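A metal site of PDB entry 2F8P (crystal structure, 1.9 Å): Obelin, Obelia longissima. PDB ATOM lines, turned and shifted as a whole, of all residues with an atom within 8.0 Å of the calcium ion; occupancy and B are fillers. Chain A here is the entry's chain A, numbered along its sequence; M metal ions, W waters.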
ATOM      1  N   LYS A   4       0.364  -7.131  13.358  1.00  0.00           N
ATOM      2  CA  LYS A   4       1.057  -7.623  12.159  1.00  0.00           C
ATOM      3  C   LYS A   4       0.568  -6.981  10.848  1.00  0.00           C
ATOM      4  O   LYS A   4       1.253  -7.087   9.851  1.00  0.00           O
ATOM      5  CB  LYS A   4       1.057  -9.145  12.066  1.00  0.00           C
ATOM      6  CG  LYS A   4      -0.314  -9.787  11.830  1.00  0.00           C
ATOM      7  CD  LYS A   4      -0.235 -11.301  11.782  1.00  0.00           C
ATOM      8  CE  LYS A   4      -0.084 -11.866  13.208  1.00  0.00           C
ATOM      9  NZ  LYS A   4      -0.023 -13.343  13.148  1.00  0.00           N
ATOM     10  N   THR A 129       5.895 -21.054   8.579  1.00  0.00           N
ATOM     11  CA  THR A 129       6.254 -20.434   9.832  1.00  0.00           C
ATOM     12  C   THR A 129       7.772 -20.460   9.962  1.00  0.00           C
ATOM     13  O   THR A 129       8.422 -21.342   9.412  1.00  0.00           O
ATOM     14  CB  THR A 129       5.616 -21.200  11.049  1.00  0.00           C
ATOM     15  OG1 THR A 129       6.043 -20.584  12.256  1.00  0.00           O
ATOM     16  CG2 THR A 129       6.094 -22.608  11.133  1.00  0.00           C
ATOM     17  N   ILE A 130       8.356 -19.479  10.648  1.00  0.00           N
ATOM     18  CA  ILE A 130       9.779 -19.564  11.016  1.00  0.00           C
ATOM     19  C   ILE A 130       9.868 -19.823  12.521  1.00  0.00           C
ATOM     20  O   ILE A 130       9.504 -18.981  13.326  1.00  0.00           O
ATOM     21  CB  ILE A 130      10.596 -18.304  10.649  1.00  0.00           C
ATOM     22  CG1 ILE A 130      10.683 -18.083   9.124  1.00  0.00           C
ATOM     23  CG2 ILE A 130      12.002 -18.385  11.253  1.00  0.00           C
ATOM     24  CD1 ILE A 130      11.178 -16.692   8.778  1.00  0.00           C
ATOM     25  N   PHE A 155      13.764 -12.264  17.690  1.00  0.00           N
ATOM     26  CA  PHE A 155      12.746 -13.271  17.402  1.00  0.00           C
ATOM     27  C   PHE A 155      11.439 -13.045  18.215  1.00  0.00           C
ATOM     28  O   PHE A 155      10.329 -13.131  17.671  1.00  0.00           O
ATOM     29  CB  PHE A 155      13.296 -14.679  17.643  1.00  0.00           C
ATOM     30  CG  PHE A 155      12.320 -15.776  17.320  1.00  0.00           C
ATOM     31  CD1 PHE A 155      12.269 -16.318  16.047  1.00  0.00           C
ATOM     32  CD2 PHE A 155      11.435 -16.241  18.291  1.00  0.00           C
ATOM     33  CE1 PHE A 155      11.358 -17.326  15.748  1.00  0.00           C
ATOM     34  CE2 PHE A 155      10.507 -17.245  17.995  1.00  0.00           C
ATOM     35  CZ  PHE A 155      10.473 -17.791  16.719  1.00  0.00           C
ATOM     36  N   ARG A 156      11.578 -12.814  19.525  1.00  0.00           N
ATOM     37  CA  ARG A 156      10.463 -12.505  20.419  1.00  0.00           C
ATOM     38  C   ARG A 156       9.773 -11.209  20.013  1.00  0.00           C
ATOM     39  O   ARG A 156       8.542 -11.060  20.120  1.00  0.00           O
ATOM     40  CB  ARG A 156      10.950 -12.403  21.877  1.00  0.00           C
ATOM     41  CG  ARG A 156      11.240 -13.750  22.564  1.00  0.00           C
ATOM     42  CD  ARG A 156      11.475 -13.611  24.103  1.00  0.00           C
ATOM     43  NE  ARG A 156      12.650 -12.780  24.420  1.00  0.00           N
ATOM     44  CZ  ARG A 156      13.897 -13.230  24.477  1.00  0.00           C
ATOM     45  NH1 ARG A 156      14.162 -14.524  24.250  1.00  0.00           N
ATOM     46  NH2 ARG A 156      14.901 -12.400  24.770  1.00  0.00           N
ATOM     47  N   CYS A 158       9.720  -9.940  16.950  1.00  0.00           N
ATOM     48  CA  CYS A 158       9.030 -10.119  15.676  1.00  0.00           C
ATOM     49  C   CYS A 158       7.784 -10.988  15.814  1.00  0.00           C
ATOM     50  O   CYS A 158       6.885 -10.946  14.987  1.00  0.00           O
ATOM     51  CB  CYS A 158       9.963 -10.750  14.644  1.00  0.00           C
ATOM     52  SG  CYS A 158      11.253  -9.650  14.040  1.00  0.00           S
ATOM     53  N   ASP A 159       7.752 -11.811  16.859  1.00  0.00           N
ATOM     54  CA  ASP A 159       6.663 -12.719  17.085  1.00  0.00           C
ATOM     55  C   ASP A 159       5.556 -11.892  17.756  1.00  0.00           C
ATOM     56  O   ASP A 159       5.426 -11.891  18.974  1.00  0.00           O
ATOM     57  CB  ASP A 159       7.118 -13.892  17.957  1.00  0.00           C
ATOM     58  CG  ASP A 159       5.982 -14.825  18.327  1.00  0.00           C
ATOM     59  OD1 ASP A 159       4.927 -14.808  17.641  1.00  0.00           O
ATOM     60  OD2 ASP A 159       6.142 -15.581  19.308  1.00  0.00           O
ATOM     61  N   LEU A 160       4.795 -11.174  16.936  1.00  0.00           N
ATOM     62  CA  LEU A 160       3.862 -10.142  17.416  1.00  0.00           C
ATOM     63  C   LEU A 160       2.670 -10.726  18.140  1.00  0.00           C
ATOM     64  O   LEU A 160       2.157 -10.120  19.093  1.00  0.00           O
ATOM     65  CB  LEU A 160       3.398  -9.228  16.261  1.00  0.00           C
ATOM     66  CG  LEU A 160       4.486  -8.406  15.566  1.00  0.00           C
ATOM     67  CD1 LEU A 160       3.957  -7.811  14.244  1.00  0.00           C
ATOM     68  CD2 LEU A 160       5.053  -7.303  16.497  1.00  0.00           C
ATOM     69  N   ASP A 161       2.206 -11.896  17.682  1.00  0.00           N
ATOM     70  CA  ASP A 161       1.031 -12.543  18.280  1.00  0.00           C
ATOM     71  C   ASP A 161       1.408 -13.604  19.326  1.00  0.00           C
ATOM     72  O   ASP A 161       0.580 -14.439  19.704  1.00  0.00           O
ATOM     73  CB  ASP A 161       0.143 -13.151  17.184  1.00  0.00           C
ATOM     74  CG  ASP A 161       0.791 -14.327  16.473  1.00  0.00           C
ATOM     75  OD1 ASP A 161       1.894 -14.743  16.905  1.00  0.00           O
ATOM     76  OD2 ASP A 161       0.192 -14.828  15.506  1.00  0.00           O
ATOM     77  N   ASN A 162       2.679 -13.546  19.752  1.00  0.00           N
ATOM     78  CA  ASN A 162       3.263 -14.470  20.748  1.00  0.00           C
ATOM     79  C   ASN A 162       2.947 -15.950  20.561  1.00  0.00           C
ATOM     80  O   ASN A 162       2.719 -16.675  21.547  1.00  0.00           O
ATOM     81  CB  ASN A 162       2.949 -13.992  22.177  1.00  0.00           C
ATOM     82  CG  ASN A 162       3.607 -12.664  22.479  1.00  0.00           C
ATOM     83  OD1 ASN A 162       2.922 -11.665  22.748  1.00  0.00           O
ATOM     84  ND2 ASN A 162       4.925 -12.629  22.385  1.00  0.00           N
ATOM     85  N   SER A 163       2.934 -16.381  19.304  1.00  0.00           N
ATOM     86  CA  SER A 163       2.678 -17.775  18.938  1.00  0.00           C
ATOM     87  C   SER A 163       3.908 -18.666  19.092  1.00  0.00           C
ATOM     88  O   SER A 163       3.807 -19.868  18.898  1.00  0.00           O
ATOM     89  CB  SER A 163       2.166 -17.866  17.493  1.00  0.00           C
ATOM     90  OG  SER A 163       3.158 -17.406  16.591  1.00  0.00           O
ATOM     91  N   GLY A 164       5.069 -18.066  19.388  1.00  0.00           N
ATOM     92  CA  GLY A 164       6.330 -18.834  19.464  1.00  0.00           C
ATOM     93  C   GLY A 164       7.017 -19.074  18.116  1.00  0.00           C
ATOM     94  O   GLY A 164       8.076 -19.690  18.073  1.00  0.00           O
ATOM     95  N   ASP A 165       6.420 -18.570  17.026  1.00  0.00           N
ATOM     96  CA  ASP A 165       7.008 -18.665  15.673  1.00  0.00           C
ATOM     97  C   ASP A 165       6.649 -17.455  14.806  1.00  0.00           C
ATOM     98  O   ASP A 165       5.722 -16.714  15.131  1.00  0.00           O
ATOM     99  CB  ASP A 165       6.621 -19.967  14.978  1.00  0.00           C
ATOM    100  CG  ASP A 165       5.098 -20.203  14.905  1.00  0.00           C
ATOM    101  OD1 ASP A 165       4.302 -19.341  15.346  1.00  0.00           O
ATOM    102  OD2 ASP A 165       4.709 -21.266  14.387  1.00  0.00           O
ATOM    103  N   LEU A 166       7.368 -17.243  13.712  1.00  0.00           N
ATOM    104  CA  LEU A 166       7.178 -16.023  12.905  1.00  0.00           C
ATOM    105  C   LEU A 166       6.420 -16.348  11.662  1.00  0.00           C
ATOM    106  O   LEU A 166       6.709 -17.355  11.007  1.00  0.00           O
ATOM    107  CB  LEU A 166       8.518 -15.408  12.531  1.00  0.00           C
ATOM    108  CG  LEU A 166       9.415 -15.014  13.694  1.00  0.00           C
ATOM    109  CD1 LEU A 166      10.696 -14.373  13.187  1.00  0.00           C
ATOM    110  CD2 LEU A 166       8.683 -14.052  14.595  1.00  0.00           C
ATOM    111  N   ASP A 167       5.417 -15.543  11.340  1.00  0.00           N
ATOM    112  CA  ASP A 167       4.789 -15.653  10.026  1.00  0.00           C
ATOM    113  C   ASP A 167       5.273 -14.541   9.084  1.00  0.00           C
ATOM    114  O   ASP A 167       5.928 -13.585   9.520  1.00  0.00           O
ATOM    115  CB  ASP A 167       3.238 -15.779  10.107  1.00  0.00           C
ATOM    116  CG  ASP A 167       2.564 -14.519  10.638  1.00  0.00           C
ATOM    117  OD1 ASP A 167       2.650 -13.456   9.990  1.00  0.00           O
ATOM    118  OD2 ASP A 167       1.918 -14.594  11.715  1.00  0.00           O
ATOM    119  N   VAL A 168       5.006 -14.693   7.794  1.00  0.00           N
ATOM    120  CA  VAL A 168       5.472 -13.715   6.818  1.00  0.00           C
ATOM    121  C   VAL A 168       4.934 -12.282   7.083  1.00  0.00           C
ATOM    122  O   VAL A 168       5.630 -11.301   6.846  1.00  0.00           O
ATOM    123  CB  VAL A 168       5.229 -14.173   5.356  1.00  0.00           C
ATOM    124  CG1 VAL A 168       3.722 -14.176   5.013  1.00  0.00           C
ATOM    125  CG2 VAL A 168       6.033 -13.279   4.405  1.00  0.00           C
ATOM    126  N   GLU A 170       4.136 -10.950  10.145  1.00  0.00           N
ATOM    127  CA  GLU A 170       4.927 -10.380  11.259  1.00  0.00           C
ATOM    128  C   GLU A 170       6.306  -9.852  10.778  1.00  0.00           C
ATOM    129  O   GLU A 170       6.665  -8.691  10.999  1.00  0.00           O
ATOM    130  CB  GLU A 170       5.110 -11.422  12.343  1.00  0.00           C
ATOM    131  CG  GLU A 170       3.860 -11.689  13.152  1.00  0.00           C
ATOM    132  CD  GLU A 170       4.001 -12.910  14.037  1.00  0.00           C
ATOM    133  OE1 GLU A 170       4.684 -13.881  13.621  1.00  0.00           O
ATOM    134  OE2 GLU A 170       3.399 -12.914  15.121  1.00  0.00           O
ATOM    135  N   MET A 171       7.059 -10.686  10.061  1.00  0.00           N
ATOM    136  CA  MET A 171       8.373 -10.312   9.574  1.00  0.00           C
ATOM    137  C   MET A 171       8.357  -9.075   8.681  1.00  0.00           C
ATOM    138  O   MET A 171       9.131  -8.150   8.930  1.00  0.00           O
ATOM    139  CB  MET A 171       9.029 -11.463   8.838  1.00  0.00           C
ATOM    140  CG  MET A 171      10.466 -11.162   8.412  1.00  0.00           C
ATOM    141  SD  MET A 171      11.223 -12.641   7.740  1.00  0.00           S
ATOM    142  CE  MET A 171      10.697 -12.425   6.051  1.00  0.00           C
HETATM  143 CA    CA M   1       3.858 -15.322  15.542  1.00  0.00          CA
HETATM  144  O   HOH W   1       2.696 -16.142  13.910  1.00  0.00           O
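Water W1 bridges the side-chain carboxylate (OD2) of Asp 167 (2.8 Å) and the side-chain carboxylate (OD2) of Asp 161 (3.2 Å).
The calcium ion is bound by water W1 (2.2 Å), the backbone carbonyl oxygen (O) of Asp 165 (2.4 Å), the side-chain carboxylate (OD1) of Asp 159 (2.4 Å), the side-chain hydroxyl (OG) of Ser 163 (2.4 Å), the side-chain carboxylate (OD1) of Asp 161 (2.5 Å), the side-chain carboxylate (OE2) of Glu 170 (2.5 Å) and the side-chain carboxylate (OE1) of Glu 170 (2.5 Å).
The calcium ion has seven donor atoms within binding distance.
Five residues have an atom within 4 Å of the calcium ion: Asp 159, Asp 161, Ser 163, Asp 165 and Glu 170.
The backbone NH (N) of Asn 162 sits close to the side-chain carboxylate (OD1) of Asp 159 (3.3 Å).
The backbone NH of Glu 170 lies within hydrogen-bond range of the side-chain carboxylate of Asp 167 (2.9 Å).
N of Leu 160 lies close to OE2 of Glu 170.
The side-chain amino group (NZ) of Lys 4 lies within salt-bridge range of the side-chain carboxylate (OD2) of Asp 161 (2.8 Å).
OE2 of Glu 170 lies close to NZ of Lys 4, at 3.97 Å.
The side-chain carboxylate of Asp 159 sits at hydrogen-bond distance from the backbone NH of Gly 164, 2.7 Å away.
The side-chain carboxylate (OD2) of Asp 165 lies within hydrogen-bond range of the side-chain hydroxyl (OG1) of Thr 129.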
